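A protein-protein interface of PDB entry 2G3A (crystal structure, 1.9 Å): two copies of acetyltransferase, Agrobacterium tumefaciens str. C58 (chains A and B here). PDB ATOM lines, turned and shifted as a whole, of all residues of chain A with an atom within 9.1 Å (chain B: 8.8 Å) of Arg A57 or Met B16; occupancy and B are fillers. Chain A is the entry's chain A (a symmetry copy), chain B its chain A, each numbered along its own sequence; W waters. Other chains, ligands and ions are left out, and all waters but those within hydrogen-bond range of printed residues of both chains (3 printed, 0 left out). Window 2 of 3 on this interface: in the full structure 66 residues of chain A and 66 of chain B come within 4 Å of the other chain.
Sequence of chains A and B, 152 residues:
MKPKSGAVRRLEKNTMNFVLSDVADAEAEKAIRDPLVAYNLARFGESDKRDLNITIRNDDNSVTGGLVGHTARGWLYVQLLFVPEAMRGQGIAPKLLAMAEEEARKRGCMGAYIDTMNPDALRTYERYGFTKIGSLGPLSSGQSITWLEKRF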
ATOM      1  N   ASN A  53      16.194  -6.559  -1.868  1.00  0.00           N
ATOM      2  CA  ASN A  53      16.700  -5.991  -3.110  1.00  0.00           C
ATOM      3  C   ASN A  53      17.611  -6.978  -3.834  1.00  0.00           C
ATOM      4  O   ASN A  53      18.283  -7.804  -3.208  1.00  0.00           O
ATOM      5  CB  ASN A  53      17.491  -4.711  -2.838  1.00  0.00           C
ATOM      6  CG  ASN A  53      16.690  -3.661  -2.086  1.00  0.00           C
ATOM      7  OD1 ASN A  53      15.489  -3.482  -2.310  1.00  0.00           O
ATOM      8  ND2 ASN A  53      17.368  -2.941  -1.199  1.00  0.00           N
ATOM      9  N   ILE A  54      17.626  -6.882  -5.156  1.00  0.00           N
ATOM     10  CA  ILE A  54      18.558  -7.632  -5.968  1.00  0.00           C
ATOM     11  C   ILE A  54      19.155  -6.623  -6.928  1.00  0.00           C
ATOM     12  O   ILE A  54      18.435  -5.998  -7.718  1.00  0.00           O
ATOM     13  CB  ILE A  54      17.888  -8.771  -6.742  1.00  0.00           C
ATOM     14  CG1 ILE A  54      17.280  -9.787  -5.774  1.00  0.00           C
ATOM     15  CG2 ILE A  54      18.903  -9.462  -7.672  1.00  0.00           C
ATOM     16  CD1 ILE A  54      16.042 -10.436  -6.294  1.00  0.00           C
ATOM     17  N   THR A  55      20.468  -6.447  -6.839  1.00  0.00           N
ATOM     18  CA  THR A  55      21.160  -5.566  -7.757  1.00  0.00           C
ATOM     19  C   THR A  55      21.873  -6.387  -8.815  1.00  0.00           C
ATOM     20  O   THR A  55      22.440  -7.440  -8.532  1.00  0.00           O
ATOM     21  CB  THR A  55      22.158  -4.627  -7.044  1.00  0.00           C
ATOM     22  OG1 THR A  55      22.924  -5.370  -6.088  1.00  0.00           O
ATOM     23  CG2 THR A  55      21.414  -3.500  -6.326  1.00  0.00           C
ATOM     24  N   ILE A  56      21.790  -5.899 -10.042  1.00  0.00           N
ATOM     25  CA  ILE A  56      22.556  -6.425 -11.151  1.00  0.00           C
ATOM     26  C   ILE A  56      23.781  -5.524 -11.258  1.00  0.00           C
ATOM     27  O   ILE A  56      23.642  -4.326 -11.493  1.00  0.00           O
ATOM     28  CB  ILE A  56      21.743  -6.366 -12.457  1.00  0.00           C
ATOM     29  CG1 ILE A  56      20.449  -7.198 -12.316  1.00  0.00           C
ATOM     30  CG2 ILE A  56      22.616  -6.823 -13.628  1.00  0.00           C
ATOM     31  CD1 ILE A  56      19.516  -7.150 -13.537  1.00  0.00           C
ATOM     32  N   ARG A  57      24.963  -6.109 -11.079  1.00  0.00           N
ATOM     33  CA  ARG A  57      26.217  -5.357 -11.015  1.00  0.00           C
ATOM     34  C   ARG A  57      27.255  -5.817 -12.047  1.00  0.00           C
ATOM     35  O   ARG A  57      27.493  -7.010 -12.217  1.00  0.00           O
ATOM     36  CB  ARG A  57      26.800  -5.419  -9.600  1.00  0.00           C
ATOM     37  CG  ARG A  57      25.952  -4.705  -8.562  1.00  0.00           C
ATOM     38  CD  ARG A  57      26.427  -5.047  -7.168  1.00  0.00           C
ATOM     39  NE  ARG A  57      25.669  -4.359  -6.121  1.00  0.00           N
ATOM     40  CZ  ARG A  57      25.943  -3.136  -5.663  1.00  0.00           C
ATOM     41  NH1 ARG A  57      26.939  -2.430  -6.180  1.00  0.00           N
ATOM     42  NH2 ARG A  57      25.199  -2.608  -4.695  1.00  0.00           N
ATOM     43  N   ASN A  58      27.861  -4.856 -12.734  1.00  0.00           N
ATOM     44  CA  ASN A  58      28.890  -5.154 -13.733  1.00  0.00           C
ATOM     45  C   ASN A  58      30.253  -5.496 -13.108  1.00  0.00           C
ATOM     46  O   ASN A  58      30.369  -5.638 -11.886  1.00  0.00           O
ATOM     47  CB  ASN A  58      29.016  -4.003 -14.747  1.00  0.00           C
ATOM     48  CG  ASN A  58      29.420  -2.671 -14.101  1.00  0.00           C
ATOM     49  OD1 ASN A  58      29.052  -1.603 -14.591  1.00  0.00           O
ATOM     50  ND2 ASN A  58      30.173  -2.731 -13.012  1.00  0.00           N
ATOM     51  N   ASP A  59      31.275  -5.614 -13.954  1.00  0.00           N
ATOM     52  CA  ASP A  59      32.630  -5.953 -13.504  1.00  0.00           C
ATOM     53  C   ASP A  59      33.264  -4.970 -12.514  1.00  0.00           C
ATOM     54  O   ASP A  59      34.137  -5.360 -11.739  1.00  0.00           O
ATOM     55  CB  ASP A  59      33.567  -6.179 -14.703  1.00  0.00           C
ATOM     56  CG  ASP A  59      33.557  -7.627 -15.197  1.00  0.00           C
ATOM     57  OD1 ASP A  59      33.997  -7.858 -16.344  1.00  0.00           O
ATOM     58  OD2 ASP A  59      33.120  -8.533 -14.448  1.00  0.00           O
ATOM     59  N   ASP A  60      32.855  -3.703 -12.549  1.00  0.00           N
ATOM     60  CA  ASP A  60      33.342  -2.736 -11.560  1.00  0.00           C
ATOM     61  C   ASP A  60      32.349  -2.422 -10.431  1.00  0.00           C
ATOM     62  O   ASP A  60      32.415  -1.358  -9.813  1.00  0.00           O
ATOM     63  CB  ASP A  60      33.906  -1.457 -12.213  1.00  0.00           C
ATOM     64  CG  ASP A  60      32.976  -0.851 -13.244  1.00  0.00           C
ATOM     65  OD1 ASP A  60      31.779  -0.658 -12.943  1.00  0.00           O
ATOM     66  OD2 ASP A  60      33.458  -0.544 -14.357  1.00  0.00           O
ATOM     67  N   ASN A  61      31.442  -3.365 -10.175  1.00  0.00           N
ATOM     68  CA  ASN A  61      30.497  -3.311  -9.048  1.00  0.00           C
ATOM     69  C   ASN A  61      29.371  -2.253  -9.164  1.00  0.00           C
ATOM     70  O   ASN A  61      28.624  -2.020  -8.207  1.00  0.00           O
ATOM     71  CB  ASN A  61      31.261  -3.198  -7.711  1.00  0.00           C
ATOM     72  CG  ASN A  61      30.416  -3.592  -6.515  1.00  0.00           C
ATOM     73  OD1 ASN A  61      29.903  -4.712  -6.440  1.00  0.00           O
ATOM     74  ND2 ASN A  61      30.264  -2.668  -5.571  1.00  0.00           N
ATOM     75  N   SER A  62      29.239  -1.631 -10.336  1.00  0.00           N
ATOM     76  CA  SER A  62      28.156  -0.665 -10.576  1.00  0.00           C
ATOM     77  C   SER A  62      26.805  -1.356 -10.753  1.00  0.00           C
ATOM     78  O   SER A  62      26.712  -2.355 -11.454  1.00  0.00           O
ATOM     79  CB  SER A  62      28.446   0.197 -11.805  1.00  0.00           C
ATOM     80  OG  SER A  62      29.298   1.280 -11.473  1.00  0.00           O
ATOM     81  N   VAL A  63      25.773  -0.797 -10.121  1.00  0.00           N
ATOM     82  CA  VAL A  63      24.392  -1.250 -10.283  1.00  0.00           C
ATOM     83  C   VAL A  63      23.856  -0.754 -11.627  1.00  0.00           C
ATOM     84  O   VAL A  63      23.836   0.455 -11.897  1.00  0.00           O
ATOM     85  CB  VAL A  63      23.488  -0.737  -9.123  1.00  0.00           C
ATOM     86  CG1 VAL A  63      22.030  -1.211  -9.282  1.00  0.00           C
ATOM     87  CG2 VAL A  63      24.052  -1.161  -7.775  1.00  0.00           C
ATOM     88  N   THR A  64      23.441  -1.701 -12.464  1.00  0.00           N
ATOM     89  CA  THR A  64      22.888  -1.404 -13.790  1.00  0.00           C
ATOM     90  C   THR A  64      21.365  -1.633 -13.833  1.00  0.00           C
ATOM     91  O   THR A  64      20.680  -1.227 -14.778  1.00  0.00           O
ATOM     92  CB  THR A  64      23.551  -2.280 -14.874  1.00  0.00           C
ATOM     93  OG1 THR A  64      23.350  -3.664 -14.558  1.00  0.00           O
ATOM     94  CG2 THR A  64      25.057  -1.996 -14.979  1.00  0.00           C
ATOM     95  N   GLY A  65      20.836  -2.281 -12.804  1.00  0.00           N
ATOM     96  CA  GLY A  65      19.418  -2.633 -12.779  1.00  0.00           C
ATOM     97  C   GLY A  65      19.122  -3.519 -11.578  1.00  0.00           C
ATOM     98  O   GLY A  65      19.953  -3.643 -10.672  1.00  0.00           O
ATOM     99  N   GLY A  66      17.946  -4.136 -11.580  1.00  0.00           N
ATOM    100  CA  GLY A  66      17.566  -5.043 -10.503  1.00  0.00           C
ATOM    101  C   GLY A  66      16.139  -4.895 -10.021  1.00  0.00           C
ATOM    102  O   GLY A  66      15.284  -4.389 -10.735  1.00  0.00           O
ATOM    103  N   PRO A  84      18.442  -3.674 -17.690  1.00  0.00           N
ATOM    104  CA  PRO A  84      19.206  -2.847 -18.636  1.00  0.00           C
ATOM    105  C   PRO A  84      18.909  -3.202 -20.097  1.00  0.00           C
ATOM    106  O   PRO A  84      18.664  -4.362 -20.425  1.00  0.00           O
ATOM    107  CB  PRO A  84      20.665  -3.173 -18.291  1.00  0.00           C
ATOM    108  CG  PRO A  84      20.625  -3.701 -16.910  1.00  0.00           C
ATOM    109  CD  PRO A  84      19.325  -4.407 -16.765  1.00  0.00           C
ATOM    110  N   ALA A  86      20.588  -3.732 -22.747  1.00  0.00           N
ATOM    111  CA  ALA A  86      21.413  -4.795 -23.337  1.00  0.00           C
ATOM    112  C   ALA A  86      21.008  -6.208 -22.899  1.00  0.00           C
ATOM    113  O   ALA A  86      21.341  -7.193 -23.571  1.00  0.00           O
ATOM    114  CB  ALA A  86      22.896  -4.549 -23.049  1.00  0.00           C
ATOM    115  N   MET A  87      20.286  -6.301 -21.782  1.00  0.00           N
ATOM    116  CA  MET A  87      19.922  -7.592 -21.217  1.00  0.00           C
ATOM    117  C   MET A  87      18.453  -7.951 -21.399  1.00  0.00           C
ATOM    118  O   MET A  87      17.958  -8.866 -20.741  1.00  0.00           O
ATOM    119  CB  MET A  87      20.262  -7.628 -19.730  1.00  0.00           C
ATOM    120  CG  MET A  87      21.701  -7.321 -19.384  1.00  0.00           C
ATOM    121  SD  MET A  87      21.850  -7.361 -17.446  1.00  0.00           S
ATOM    122  CE  MET A  87      22.033  -9.322 -17.160  1.00  0.00           C
ATOM    123  N   GLN A  90      15.723 -11.859 -22.445  1.00  0.00           N
ATOM    124  CA  GLN A  90      16.700 -12.870 -22.041  1.00  0.00           C
ATOM    125  C   GLN A  90      16.346 -13.500 -20.686  1.00  0.00           C
ATOM    126  O   GLN A  90      17.211 -14.046 -19.999  1.00  0.00           O
ATOM    127  CB  GLN A  90      18.105 -12.235 -21.996  1.00  0.00           C
ATOM    128  CG  GLN A  90      18.718 -11.994 -23.383  1.00  0.00           C
ATOM    129  CD  GLN A  90      19.831 -10.960 -23.394  1.00  0.00           C
ATOM    130  OE1 GLN A  90      20.786 -11.045 -22.622  1.00  0.00           O
ATOM    131  NE2 GLN A  90      19.715  -9.978 -24.289  1.00  0.00           N
ATOM    132  N   ILE A  92      15.614 -12.098 -17.887  1.00  0.00           N
ATOM    133  CA  ILE A  92      16.212 -11.432 -16.733  1.00  0.00           C
ATOM    134  C   ILE A  92      15.170 -10.932 -15.728  1.00  0.00           C
ATOM    135  O   ILE A  92      15.360 -11.078 -14.523  1.00  0.00           O
ATOM    136  CB  ILE A  92      17.179 -10.279 -17.130  1.00  0.00           C
ATOM    137  CG1 ILE A  92      18.334 -10.804 -17.977  1.00  0.00           C
ATOM    138  CG2 ILE A  92      17.682  -9.534 -15.865  1.00  0.00           C
ATOM    139  CD1 ILE A  92      19.081 -11.994 -17.387  1.00  0.00           C
ATOM    140  N   LYS A  95      14.016 -13.855 -13.926  1.00  0.00           N
ATOM    141  CA  LYS A  95      15.080 -14.307 -13.032  1.00  0.00           C
ATOM    142  C   LYS A  95      15.065 -13.514 -11.732  1.00  0.00           C
ATOM    143  O   LYS A  95      15.242 -14.081 -10.656  1.00  0.00           O
ATOM    144  CB  LYS A  95      16.452 -14.209 -13.708  1.00  0.00           C
ATOM    145  CG  LYS A  95      17.623 -14.596 -12.792  1.00  0.00           C
ATOM    146  CD  LYS A  95      18.913 -14.756 -13.579  1.00  0.00           C
ATOM    147  CE  LYS A  95      20.047 -15.279 -12.691  1.00  0.00           C
ATOM    148  NZ  LYS A  95      21.278 -15.499 -13.506  1.00  0.00           N
ATOM    149  N   LEU A  96      14.889 -12.198 -11.845  1.00  0.00           N
ATOM    150  CA  LEU A  96      14.778 -11.327 -10.678  1.00  0.00           C
ATOM    151  C   LEU A  96      13.560 -11.696  -9.850  1.00  0.00           C
ATOM    152  O   LEU A  96      13.657 -11.796  -8.632  1.00  0.00           O
ATOM    153  CB  LEU A  96      14.712  -9.847 -11.095  1.00  0.00           C
ATOM    154  CG  LEU A  96      15.977  -9.267 -11.743  1.00  0.00           C
ATOM    155  CD1 LEU A  96      15.649  -7.970 -12.437  1.00  0.00           C
ATOM    156  CD2 LEU A  96      17.103  -9.071 -10.727  1.00  0.00           C
ATOM    157  N   MET A  99      14.305 -14.990  -8.043  1.00  0.00           N
ATOM    158  CA  MET A  99      15.205 -14.797  -6.897  1.00  0.00           C
ATOM    159  C   MET A  99      14.487 -14.173  -5.700  1.00  0.00           C
ATOM    160  O   MET A  99      14.708 -14.573  -4.546  1.00  0.00           O
ATOM    161  CB  MET A  99      16.398 -13.938  -7.288  1.00  0.00           C
ATOM    162  CG  MET A  99      17.318 -14.610  -8.294  1.00  0.00           C
ATOM    163  SD  MET A  99      18.819 -13.451  -8.710  1.00  0.00           S
ATOM    164  CE  MET A  99      19.591 -13.198  -6.905  1.00  0.00           C
ATOM    165  N   MET B  16      28.000 -10.809 -15.391  1.00  0.00           N
ATOM    166  CA  MET B  16      27.028  -9.959 -14.651  1.00  0.00           C
ATOM    167  C   MET B  16      26.629 -10.624 -13.335  1.00  0.00           C
ATOM    168  O   MET B  16      26.243 -11.794 -13.316  1.00  0.00           O
ATOM    169  CB  MET B  16      25.794  -9.703 -15.518  1.00  0.00           C
ATOM    170  CG  MET B  16      25.204  -8.307 -15.391  1.00  0.00           C
ATOM    171  SD  MET B  16      26.309  -6.835 -16.104  1.00  0.00           S
ATOM    172  CE  MET B  16      26.742  -7.572 -17.888  1.00  0.00           C
ATOM    173  N   ASN B  17      26.724  -9.874 -12.239  1.00  0.00           N
ATOM    174  CA  ASN B  17      26.447 -10.407 -10.900  1.00  0.00           C
ATOM    175  C   ASN B  17      25.093  -9.995 -10.345  1.00  0.00           C
ATOM    176  O   ASN B  17      24.764  -8.813 -10.330  1.00  0.00           O
ATOM    177  CB  ASN B  17      27.534  -9.971  -9.908  1.00  0.00           C
ATOM    178  CG  ASN B  17      28.886 -10.499 -10.274  1.00  0.00           C
ATOM    179  OD1 ASN B  17      29.828  -9.732 -10.479  1.00  0.00           O
ATOM    180  ND2 ASN B  17      28.994 -11.819 -10.377  1.00  0.00           N
ATOM    181  N   PHE B  18      24.334 -10.979  -9.868  1.00  0.00           N
ATOM    182  CA  PHE B  18      23.033 -10.746  -9.241  1.00  0.00           C
ATOM    183  C   PHE B  18      23.184 -10.888  -7.728  1.00  0.00           C
ATOM    184  O   PHE B  18      23.458 -11.980  -7.216  1.00  0.00           O
ATOM    185  CB  PHE B  18      21.992 -11.738  -9.765  1.00  0.00           C
ATOM    186  CG  PHE B  18      21.610 -11.529 -11.209  1.00  0.00           C
ATOM    187  CD1 PHE B  18      20.365 -10.991 -11.534  1.00  0.00           C
ATOM    188  CD2 PHE B  18      22.472 -11.900 -12.239  1.00  0.00           C
ATOM    189  CE1 PHE B  18      19.984 -10.815 -12.857  1.00  0.00           C
ATOM    190  CE2 PHE B  18      22.114 -11.720 -13.571  1.00  0.00           C
ATOM    191  CZ  PHE B  18      20.865 -11.177 -13.887  1.00  0.00           C
ATOM    192  N   VAL B  19      23.015  -9.776  -7.017  1.00  0.00           N
ATOM    193  CA  VAL B  19      23.328  -9.711  -5.582  1.00  0.00           C
ATOM    194  C   VAL B  19      22.052  -9.486  -4.786  1.00  0.00           C
ATOM    195  O   VAL B  19      21.388  -8.466  -4.959  1.00  0.00           O
ATOM    196  CB  VAL B  19      24.313  -8.560  -5.266  1.00  0.00           C
ATOM    197  CG1 VAL B  19      24.660  -8.542  -3.771  1.00  0.00           C
ATOM    198  CG2 VAL B  19      25.573  -8.681  -6.109  1.00  0.00           C
ATOM    199  N   LEU B  20      21.712 -10.446  -3.928  1.00  0.00           N
ATOM    200  CA  LEU B  20      20.534 -10.339  -3.062  1.00  0.00           C
ATOM    201  C   LEU B  20      20.915  -9.617  -1.779  1.00  0.00           C
ATOM    202  O   LEU B  20      21.973  -9.881  -1.216  1.00  0.00           O
ATOM    203  CB  LEU B  20      19.987 -11.728  -2.731  1.00  0.00           C
ATOM    204  CG  LEU B  20      18.793 -11.818  -1.772  1.00  0.00           C
ATOM    205  CD1 LEU B  20      17.549 -11.213  -2.388  1.00  0.00           C
ATOM    206  CD2 LEU B  20      18.534 -13.264  -1.380  1.00  0.00           C
ATOM    207  N   SER B  21      20.060  -8.709  -1.323  1.00  0.00           N
ATOM    208  CA  SER B  21      20.319  -7.963  -0.082  1.00  0.00           C
ATOM    209  C   SER B  21      19.021  -7.698   0.695  1.00  0.00           C
ATOM    210  O   SER B  21      17.944  -7.605   0.098  1.00  0.00           O
ATOM    211  CB  SER B  21      21.036  -6.647  -0.407  1.00  0.00           C
ATOM    212  OG  SER B  21      21.413  -5.953   0.763  1.00  0.00           O
ATOM    213  N   ASP B  25      19.418   0.658   1.074  1.00  0.00           N
ATOM    214  CA  ASP B  25      20.571   1.240   0.388  1.00  0.00           C
ATOM    215  C   ASP B  25      20.077   2.296  -0.587  1.00  0.00           C
ATOM    216  O   ASP B  25      19.558   1.964  -1.659  1.00  0.00           O
ATOM    217  CB  ASP B  25      21.345   0.152  -0.366  1.00  0.00           C
ATOM    218  CG  ASP B  25      22.735   0.605  -0.799  1.00  0.00           C
ATOM    219  OD1 ASP B  25      23.177   1.711  -0.412  1.00  0.00           O
ATOM    220  OD2 ASP B  25      23.397  -0.165  -1.525  1.00  0.00           O
ATOM    221  N   GLU B  27      21.669   4.630  -2.475  1.00  0.00           N
ATOM    222  CA  GLU B  27      22.385   4.716  -3.753  1.00  0.00           C
ATOM    223  C   GLU B  27      22.100   3.554  -4.698  1.00  0.00           C
ATOM    224  O   GLU B  27      22.036   3.747  -5.915  1.00  0.00           O
ATOM    225  CB  GLU B  27      23.893   4.858  -3.535  1.00  0.00           C
ATOM    226  CG  GLU B  27      24.335   6.275  -3.203  1.00  0.00           C
ATOM    227  CD  GLU B  27      24.316   6.572  -1.699  1.00  0.00           C
ATOM    228  OE1 GLU B  27      23.499   5.938  -0.947  1.00  0.00           O
ATOM    229  OE2 GLU B  27      25.124   7.446  -1.267  1.00  0.00           O
ATOM    230  N   ALA B  28      21.933   2.355  -4.145  1.00  0.00           N
ATOM    231  CA  ALA B  28      21.594   1.192  -4.952  1.00  0.00           C
ATOM    232  C   ALA B  28      20.161   1.306  -5.464  1.00  0.00           C
ATOM    233  O   ALA B  28      19.891   1.035  -6.634  1.00  0.00           O
ATOM    234  CB  ALA B  28      21.777  -0.086  -4.162  1.00  0.00           C
ATOM    235  N   GLU B  29      19.253   1.728  -4.584  1.00  0.00           N
ATOM    236  CA  GLU B  29      17.851   1.919  -4.947  1.00  0.00           C
ATOM    237  C   GLU B  29      17.661   3.030  -5.976  1.00  0.00           C
ATOM    238  O   GLU B  29      16.813   2.909  -6.857  1.00  0.00           O
ATOM    239  CB  GLU B  29      17.005   2.201  -3.713  1.00  0.00           C
ATOM    240  CG  GLU B  29      16.667   0.958  -2.915  1.00  0.00           C
ATOM    241  CD  GLU B  29      15.793   1.263  -1.719  1.00  0.00           C
ATOM    242  OE1 GLU B  29      14.684   1.817  -1.909  1.00  0.00           O
ATOM    243  OE2 GLU B  29      16.219   0.945  -0.589  1.00  0.00           O
ATOM    244  N   ALA B  31      19.972   3.859  -8.190  1.00  0.00           N
ATOM    245  CA  ALA B  31      20.582   3.339  -9.414  1.00  0.00           C
ATOM    246  C   ALA B  31      19.644   2.421 -10.199  1.00  0.00           C
ATOM    247  O   ALA B  31      19.891   2.139 -11.370  1.00  0.00           O
ATOM    248  CB  ALA B  31      21.879   2.612  -9.093  1.00  0.00           C
ATOM    249  N   ILE B  32      18.586   1.955  -9.542  1.00  0.00           N
ATOM    250  CA  ILE B  32      17.525   1.166 -10.190  1.00  0.00           C
ATOM    251  C   ILE B  32      16.332   2.062 -10.551  1.00  0.00           C
ATOM    252  O   ILE B  32      15.787   1.960 -11.647  1.00  0.00           O
ATOM    253  CB  ILE B  32      17.062  -0.007  -9.281  1.00  0.00           C
ATOM    254  CG1 ILE B  32      18.203  -1.011  -9.077  1.00  0.00           C
ATOM    255  CG2 ILE B  32      15.834  -0.713  -9.874  1.00  0.00           C
ATOM    256  CD1 ILE B  32      17.925  -2.053  -8.001  1.00  0.00           C
HETATM  257  O   HOH W   1      30.304  -7.141  -9.249  1.00  0.00           O
HETATM  258  O   HOH W   2      21.655  -5.912  -3.649  1.00  0.00           O
HETATM  259  O   HOH W   3      22.019   2.841 -12.793  1.00  0.00           O
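No position is printed for both chains.
Water W3 bridges O of Ala B31 (2.7 Å) and O of Val A63 (3.1 Å). Water W2 lies within hydrogen-bond range of the side-chain hydroxyl (OG1) of Thr A55 (2.8 Å) and the backbone carbonyl oxygen (O) of Val B19 (2.9 Å). Water W1 lies within hydrogen-bond range of OD1 of Asn B17 and O of Asn A58.
Of chain B, only Met B16, Asn B17 and Val B19 come within 4 Å of Arg A57. Of the printed residues of chain B, Gly A65 touches Ile B32. Printed residues of chain B within 4 Å of Ile A92: Phe B18. Met B16 touches four residues of chain A. Of chain A, only Thr A55, Ile A56 and Arg A57 come within 4 Å of Asn B17. Of the printed residues of chain A, Ala B31 touches Val A63. The nearest residue of chain A that does not touch Met B16 is Thr A64 (4.6 Å). The nearest printed residue of chain A that does not touch Ser B21 is Ile A54 (4.9 Å).
O of Val B19 touches O of Asn A53 (3.6 Å). Asn A53 touches Leu B20. Ile A54 touches Val B19. Leu B20 touches Ile A54 (CD1 to CG1, 3.7 Å). Arg A57 touches Met B16. CD of Arg A57 touches CG2 of Val B19, at 3.9 Å. Met B16 touches Asn A58. O of Gly A65 touches CG1 of Ile B32 (3.5 Å). CZ of Phe B18 touches CE of Met A87, at 3.9 Å. Lys A95 touches Phe B18.
Of the 12 printed residues of chain B, 8 touch a printed residue of chain A. Hydrophobic or aromatic side chains of chain B that line the printed part of chain A: Met B16, Phe B18, Val B19, Leu B20, Ala B31 and Ile B32. Along chain B the printed residues that touch a printed residue of chain A span positions 16 to 32. Printed residues of chain A that touch a printed residue of chain B: Asn A53, Ile A54, Thr A55, Ile A56, Arg A57, Asn A58, Val A63, Gly A65, Gly A66, Met A87, Ile A92, Lys A95, Leu A96 and Met A99. Among the printed residues, 26 pairs touch across the chains. Among the printed residues, no Asp or Glu carboxylate lies within 4 Å of a Lys or Arg side-chain nitrogen of the other chain.
The backbone NH (N) of Ser B21 lies within hydrogen-bond range of the backbone carbonyl oxygen (O) of Asn A53. The backbone carbonyl oxygen (O) of Thr A55 lies close to the backbone carbonyl oxygen (O) of Asn B17. The backbone carbonyl oxygen (O) of Thr A55 lies within hydrogen-bond range of the backbone NH (N) of Val B19 (2.8 Å). O of Asn B17 sits at hydrogen-bond distance from N of Arg A57, at 2.8 Å.
The backbone carbonyl oxygen of Gly A65 is in hydrogen-bond range of the backbone NH of Ile A56 (3.0 Å). The guanidinium group of Arg A57 sits at hydrogen-bond distance from the side-chain hydroxyl of Thr A55 (2.9 Å). The backbone NH (N) of Ser A62 sits close to the side-chain amide nitrogen (ND2) of Asn A58, at 3.0 Å. The side-chain amide nitrogen (ND2) of Asn A58 is in hydrogen-bond range of the side-chain carboxylate (OD1) of Asp A60 (2.6 Å). N of Asn A61 sits close to ND2 of Asn A58 (3.2 Å). The backbone carbonyl oxygen (O) of Asn A61 sits at hydrogen-bond distance from the guanidinium group (NH1) of Arg A57, 2.7 Å away.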
